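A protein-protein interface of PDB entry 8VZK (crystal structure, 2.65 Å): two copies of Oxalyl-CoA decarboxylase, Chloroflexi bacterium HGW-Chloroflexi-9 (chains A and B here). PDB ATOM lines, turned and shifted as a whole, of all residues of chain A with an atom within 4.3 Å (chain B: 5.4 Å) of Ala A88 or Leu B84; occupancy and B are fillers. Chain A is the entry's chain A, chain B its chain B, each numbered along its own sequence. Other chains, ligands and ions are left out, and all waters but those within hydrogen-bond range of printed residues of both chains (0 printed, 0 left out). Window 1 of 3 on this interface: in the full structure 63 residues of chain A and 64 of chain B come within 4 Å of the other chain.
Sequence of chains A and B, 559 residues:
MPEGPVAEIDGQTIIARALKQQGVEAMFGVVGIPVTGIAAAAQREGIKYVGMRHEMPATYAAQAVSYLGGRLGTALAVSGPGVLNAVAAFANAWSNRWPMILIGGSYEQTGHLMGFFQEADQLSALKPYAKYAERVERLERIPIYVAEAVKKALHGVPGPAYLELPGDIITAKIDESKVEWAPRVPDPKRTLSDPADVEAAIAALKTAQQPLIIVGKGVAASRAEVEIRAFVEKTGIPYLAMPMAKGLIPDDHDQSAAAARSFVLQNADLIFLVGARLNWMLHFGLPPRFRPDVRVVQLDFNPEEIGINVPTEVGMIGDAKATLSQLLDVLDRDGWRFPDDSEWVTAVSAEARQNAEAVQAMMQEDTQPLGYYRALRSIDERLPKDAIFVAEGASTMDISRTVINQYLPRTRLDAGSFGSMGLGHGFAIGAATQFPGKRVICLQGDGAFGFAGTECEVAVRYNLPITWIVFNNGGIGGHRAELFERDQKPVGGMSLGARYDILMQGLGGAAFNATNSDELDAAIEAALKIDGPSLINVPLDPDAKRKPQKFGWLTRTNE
OH of Tyr A129 sits at hydrogen-bond distance from O of Asp B121 (2.6 Å). The backbone carbonyl oxygen (O) of Leu B84 sits at hydrogen-bond distance from the backbone NH (N) of Ala A88 (3.3 Å).
The backbone NH (N) of Gly B80 sits at hydrogen-bond distance from the side-chain amide oxygen (OE1) of Gln B122, 2.8 Å away.
Val A87 touches Leu B84 (CB to O, 3.7 Å). CB of Val A87 touches CG2 of Val B87, 3.8 Å away. Ala A88 touches Pro B81. CB of Ala A88 touches OD1 of Asn B85, 3.2 Å away. Ala A91 touches Leu B84 (CB to CD1, 3.6 Å). Tyr A129 touches Leu B84 (OH to CD2, 3.3 Å). Tyr A129 touches Gln B122. OH of Tyr A129 touches CB of Ala B125 (3.3 Å).
Of chain B, only Pro B81, Leu B84 and Asn B85 come within 4 Å of Ala A88. Printed residues of chain B within 4 Å of Ala A91: Leu B84. Gly B80 touches none of the printed residues of chain A. Leu B84 touches just these residues of chain A: Val A87, Ala A88, Ala A91 and Tyr A129. Of the printed residues of chain A, Asp B121 touches Tyr A129. Of the printed residues of chain A, Gln B122 touches Tyr A129 (3.7 Å). The nearest printed residue of chain B that does not touch Ala A88 is Gly B80 (5.4 Å). The nearest printed residue of chain A that does not touch Leu B84 is Ala A86 (5.3 Å). The nearest printed residue of chain A that does not touch Pro B81 is Tyr A60 (5.0 Å).
Of the 9 printed residues of chain A, 4 touch a printed residue of chain B. Printed residues of chain A that touch a printed residue of chain B: Val A87, Ala A88, Ala A91 and Tyr A129. Hydrophobic or aromatic side chains of chain A that line the printed part of chain B: Val A87, Ala A88, Ala A91 and Tyr A129. Along chain A the printed residues that touch a printed residue of chain B span positions 87 to 129. Hydrophobic or aromatic side chains of chain B within 4 Å of the printed part of chain A: Leu B84, Val B87 and Ala B125. Among the printed residues, no Asp or Glu carboxylate lies within 4 Å of a Lys or Arg side-chain nitrogen of the other chain.
Val B87 touches its own counterpart, Val A87. Positions printed for both chains: 86 and 87.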
ATOM      1  N   TYR A  60     -26.246  -2.765  11.201  1.00  0.00           N
ATOM      2  CA  TYR A  60     -27.646  -2.953  10.831  1.00  0.00           C
ATOM      3  C   TYR A  60     -28.003  -2.163   9.580  1.00  0.00           C
ATOM      4  O   TYR A  60     -28.832  -2.612   8.779  1.00  0.00           O
ATOM      5  CB  TYR A  60     -28.563  -2.549  11.985  1.00  0.00           C
ATOM      6  CG  TYR A  60     -28.621  -3.549  13.115  1.00  0.00           C
ATOM      7  CD1 TYR A  60     -29.023  -4.860  12.890  1.00  0.00           C
ATOM      8  CD2 TYR A  60     -28.294  -3.178  14.412  1.00  0.00           C
ATOM      9  CE1 TYR A  60     -29.084  -5.776  13.923  1.00  0.00           C
ATOM     10  CE2 TYR A  60     -28.354  -4.085  15.451  1.00  0.00           C
ATOM     11  CZ  TYR A  60     -28.748  -5.382  15.202  1.00  0.00           C
ATOM     12  OH  TYR A  60     -28.806  -6.285  16.238  1.00  0.00           O
ATOM     13  N   ALA A  86     -20.083  -4.858  17.074  1.00  0.00           N
ATOM     14  CA  ALA A  86     -21.052  -5.186  16.038  1.00  0.00           C
ATOM     15  C   ALA A  86     -21.300  -6.687  15.927  1.00  0.00           C
ATOM     16  O   ALA A  86     -21.819  -7.150  14.907  1.00  0.00           O
ATOM     17  CB  ALA A  86     -20.595  -4.626  14.692  1.00  0.00           C
ATOM     18  N   VAL A  87     -20.943  -7.457  16.957  1.00  0.00           N
ATOM     19  CA  VAL A  87     -21.120  -8.904  16.895  1.00  0.00           C
ATOM     20  C   VAL A  87     -22.601  -9.264  16.873  1.00  0.00           C
ATOM     21  O   VAL A  87     -23.016 -10.197  16.174  1.00  0.00           O
ATOM     22  CB  VAL A  87     -20.387  -9.582  18.066  1.00  0.00           C
ATOM     23  CG1 VAL A  87     -20.629 -11.083  18.051  1.00  0.00           C
ATOM     24  CG2 VAL A  87     -18.898  -9.283  18.001  1.00  0.00           C
ATOM     25  N   ALA A  88     -23.421  -8.533  17.631  1.00  0.00           N
ATOM     26  CA  ALA A  88     -24.852  -8.821  17.660  1.00  0.00           C
ATOM     27  C   ALA A  88     -25.506  -8.482  16.327  1.00  0.00           C
ATOM     28  O   ALA A  88     -26.289  -9.273  15.789  1.00  0.00           O
ATOM     29  CB  ALA A  88     -25.520  -8.057  18.802  1.00  0.00           C
ATOM     30  N   ALA A  89     -25.196  -7.307  15.777  1.00  0.00           N
ATOM     31  CA  ALA A  89     -25.714  -6.957  14.460  1.00  0.00           C
ATOM     32  C   ALA A  89     -25.174  -7.890  13.386  1.00  0.00           C
ATOM     33  O   ALA A  89     -25.861  -8.161  12.395  1.00  0.00           O
ATOM     34  CB  ALA A  89     -25.374  -5.504  14.131  1.00  0.00           C
ATOM     35  N   PHE A  90     -23.950  -8.390  13.568  1.00  0.00           N
ATOM     36  CA  PHE A  90     -23.398  -9.371  12.638  1.00  0.00           C
ATOM     37  C   PHE A  90     -24.170 -10.681  12.707  1.00  0.00           C
ATOM     38  O   PHE A  90     -24.441 -11.305  11.675  1.00  0.00           O
ATOM     39  CB  PHE A  90     -21.919  -9.599  12.949  1.00  0.00           C
ATOM     40  CG  PHE A  90     -21.155 -10.272  11.846  1.00  0.00           C
ATOM     41  CD1 PHE A  90     -20.550  -9.524  10.850  1.00  0.00           C
ATOM     42  CD2 PHE A  90     -21.022 -11.649  11.817  1.00  0.00           C
ATOM     43  CE1 PHE A  90     -19.838 -10.137   9.837  1.00  0.00           C
ATOM     44  CE2 PHE A  90     -20.312 -12.267  10.809  1.00  0.00           C
ATOM     45  CZ  PHE A  90     -19.717 -11.510   9.819  1.00  0.00           C
ATOM     46  N   ALA A  91     -24.537 -11.110  13.918  1.00  0.00           N
ATOM     47  CA  ALA A  91     -25.300 -12.342  14.071  1.00  0.00           C
ATOM     48  C   ALA A  91     -26.732 -12.185  13.581  1.00  0.00           C
ATOM     49  O   ALA A  91     -27.338 -13.161  13.124  1.00  0.00           O
ATOM     50  CB  ALA A  91     -25.289 -12.787  15.533  1.00  0.00           C
ATOM     51  N   ASN A  92     -27.293 -10.977  13.674  1.00  0.00           N
ATOM     52  CA  ASN A  92     -28.649 -10.759  13.184  1.00  0.00           C
ATOM     53  C   ASN A  92     -28.725 -10.963  11.677  1.00  0.00           C
ATOM     54  O   ASN A  92     -29.714 -11.499  11.163  1.00  0.00           O
ATOM     55  CB  ASN A  92     -29.128  -9.358  13.567  1.00  0.00           C
ATOM     56  CG  ASN A  92     -30.554  -9.090  13.128  1.00  0.00           C
ATOM     57  OD1 ASN A  92     -31.506  -9.429  13.830  1.00  0.00           O
ATOM     58  ND2 ASN A  92     -30.708  -8.474  11.962  1.00  0.00           N
ATOM     59  N   TYR A 129     -20.814 -17.016  13.071  1.00  0.00           N
ATOM     60  CA  TYR A 129     -21.955 -16.525  12.316  1.00  0.00           C
ATOM     61  C   TYR A 129     -21.610 -16.125  10.888  1.00  0.00           C
ATOM     62  O   TYR A 129     -22.520 -15.788  10.123  1.00  0.00           O
ATOM     63  CB  TYR A 129     -22.591 -15.320  13.032  1.00  0.00           C
ATOM     64  CG  TYR A 129     -22.462 -15.375  14.537  1.00  0.00           C
ATOM     65  CD1 TYR A 129     -23.329 -16.145  15.300  1.00  0.00           C
ATOM     66  CD2 TYR A 129     -21.469 -14.660  15.194  1.00  0.00           C
ATOM     67  CE1 TYR A 129     -23.212 -16.202  16.676  1.00  0.00           C
ATOM     68  CE2 TYR A 129     -21.344 -14.709  16.569  1.00  0.00           C
ATOM     69  CZ  TYR A 129     -22.218 -15.482  17.305  1.00  0.00           C
ATOM     70  OH  TYR A 129     -22.099 -15.536  18.675  1.00  0.00           O
ATOM     71  N   GLY B  80     -29.124 -14.271  22.943  1.00  0.00           N
ATOM     72  CA  GLY B  80     -28.870 -13.921  21.566  1.00  0.00           C
ATOM     73  C   GLY B  80     -28.269 -12.541  21.387  1.00  0.00           C
ATOM     74  O   GLY B  80     -27.102 -12.297  21.709  1.00  0.00           O
ATOM     75  N   PRO B  81     -29.062 -11.610  20.849  1.00  0.00           N
ATOM     76  CA  PRO B  81     -28.546 -10.250  20.615  1.00  0.00           C
ATOM     77  C   PRO B  81     -28.084  -9.543  21.876  1.00  0.00           C
ATOM     78  O   PRO B  81     -27.158  -8.725  21.809  1.00  0.00           O
ATOM     79  CB  PRO B  81     -29.741  -9.529  19.977  1.00  0.00           C
ATOM     80  CG  PRO B  81     -30.575 -10.614  19.394  1.00  0.00           C
ATOM     81  CD  PRO B  81     -30.415 -11.794  20.296  1.00  0.00           C
ATOM     82  N   GLY B  82     -28.701  -9.829  23.025  1.00  0.00           N
ATOM     83  CA  GLY B  82     -28.307  -9.152  24.250  1.00  0.00           C
ATOM     84  C   GLY B  82     -26.884  -9.471  24.663  1.00  0.00           C
ATOM     85  O   GLY B  82     -26.089  -8.572  24.948  1.00  0.00           O
ATOM     86  N   VAL B  83     -26.540 -10.760  24.695  1.00  0.00           N
ATOM     87  CA  VAL B  83     -25.188 -11.159  25.076  1.00  0.00           C
ATOM     88  C   VAL B  83     -24.175 -10.669  24.052  1.00  0.00           C
ATOM     89  O   VAL B  83     -23.106 -10.158  24.409  1.00  0.00           O
ATOM     90  CB  VAL B  83     -25.114 -12.686  25.261  1.00  0.00           C
ATOM     91  CG1 VAL B  83     -23.686 -13.116  25.553  1.00  0.00           C
ATOM     92  CG2 VAL B  83     -26.042 -13.128  26.377  1.00  0.00           C
ATOM     93  N   LEU B  84     -24.493 -10.805  22.763  1.00  0.00           N
ATOM     94  CA  LEU B  84     -23.565 -10.409  21.713  1.00  0.00           C
ATOM     95  C   LEU B  84     -23.445  -8.897  21.566  1.00  0.00           C
ATOM     96  O   LEU B  84     -22.588  -8.433  20.806  1.00  0.00           O
ATOM     97  CB  LEU B  84     -23.989 -11.034  20.386  1.00  0.00           C
ATOM     98  CG  LEU B  84     -24.090 -12.560  20.403  1.00  0.00           C
ATOM     99  CD1 LEU B  84     -24.451 -13.091  19.028  1.00  0.00           C
ATOM    100  CD2 LEU B  84     -22.793 -13.183  20.899  1.00  0.00           C
ATOM    101  N   ASN B  85     -24.274  -8.123  22.267  1.00  0.00           N
ATOM    102  CA  ASN B  85     -24.147  -6.672  22.267  1.00  0.00           C
ATOM    103  C   ASN B  85     -23.034  -6.178  23.180  1.00  0.00           C
ATOM    104  O   ASN B  85     -22.707  -4.986  23.140  1.00  0.00           O
ATOM    105  CB  ASN B  85     -25.471  -6.030  22.687  1.00  0.00           C
ATOM    106  CG  ASN B  85     -26.136  -5.273  21.558  1.00  0.00           C
ATOM    107  OD1 ASN B  85     -25.695  -5.329  20.411  1.00  0.00           O
ATOM    108  ND2 ASN B  85     -27.209  -4.560  21.878  1.00  0.00           N
ATOM    109  N   ALA B  86     -22.447  -7.056  23.994  1.00  0.00           N
ATOM    110  CA  ALA B  86     -21.444  -6.664  24.977  1.00  0.00           C
ATOM    111  C   ALA B  86     -20.111  -7.373  24.760  1.00  0.00           C
ATOM    112  O   ALA B  86     -19.320  -7.493  25.701  1.00  0.00           O
ATOM    113  CB  ALA B  86     -21.956  -6.929  26.392  1.00  0.00           C
ATOM    114  N   VAL B  87     -19.843  -7.843  23.540  1.00  0.00           N
ATOM    115  CA  VAL B  87     -18.593  -8.549  23.280  1.00  0.00           C
ATOM    116  C   VAL B  87     -17.404  -7.606  23.422  1.00  0.00           C
ATOM    117  O   VAL B  87     -16.363  -7.979  23.976  1.00  0.00           O
ATOM    118  CB  VAL B  87     -18.633  -9.209  21.889  1.00  0.00           C
ATOM    119  CG1 VAL B  87     -17.321  -9.922  21.602  1.00  0.00           C
ATOM    120  CG2 VAL B  87     -19.801 -10.179  21.798  1.00  0.00           C
ATOM    121  N   ASP B 121     -25.301 -19.606  18.834  1.00  0.00           N
ATOM    122  CA  ASP B 121     -24.061 -19.955  19.524  1.00  0.00           C
ATOM    123  C   ASP B 121     -23.428 -18.660  20.015  1.00  0.00           C
ATOM    124  O   ASP B 121     -22.605 -18.044  19.336  1.00  0.00           O
ATOM    125  CB  ASP B 121     -23.125 -20.731  18.605  1.00  0.00           C
ATOM    126  CG  ASP B 121     -21.854 -21.182  19.305  1.00  0.00           C
ATOM    127  OD1 ASP B 121     -21.755 -21.017  20.540  1.00  0.00           O
ATOM    128  OD2 ASP B 121     -20.951 -21.703  18.616  1.00  0.00           O
ATOM    129  N   GLN B 122     -23.828 -18.237  21.209  1.00  0.00           N
ATOM    130  CA  GLN B 122     -23.241 -17.068  21.845  1.00  0.00           C
ATOM    131  C   GLN B 122     -22.079 -17.422  22.761  1.00  0.00           C
ATOM    132  O   GLN B 122     -21.321 -16.528  23.151  1.00  0.00           O
ATOM    133  CB  GLN B 122     -24.314 -16.307  22.631  1.00  0.00           C
ATOM    134  CG  GLN B 122     -25.085 -17.167  23.617  1.00  0.00           C
ATOM    135  CD  GLN B 122     -26.421 -16.561  23.993  1.00  0.00           C
ATOM    136  OE1 GLN B 122     -27.298 -16.391  23.147  1.00  0.00           O
ATOM    137  NE2 GLN B 122     -26.583 -16.227  25.268  1.00  0.00           N
ATOM    138  N   ALA B 125     -18.565 -16.810  21.024  1.00  0.00           N
ATOM    139  CA  ALA B 125     -18.161 -15.436  20.747  1.00  0.00           C
ATOM    140  C   ALA B 125     -17.412 -14.798  21.909  1.00  0.00           C
ATOM    141  O   ALA B 125     -16.679 -13.826  21.696  1.00  0.00           O
ATOM    142  CB  ALA B 125     -19.384 -14.590  20.393  1.00  0.00           C
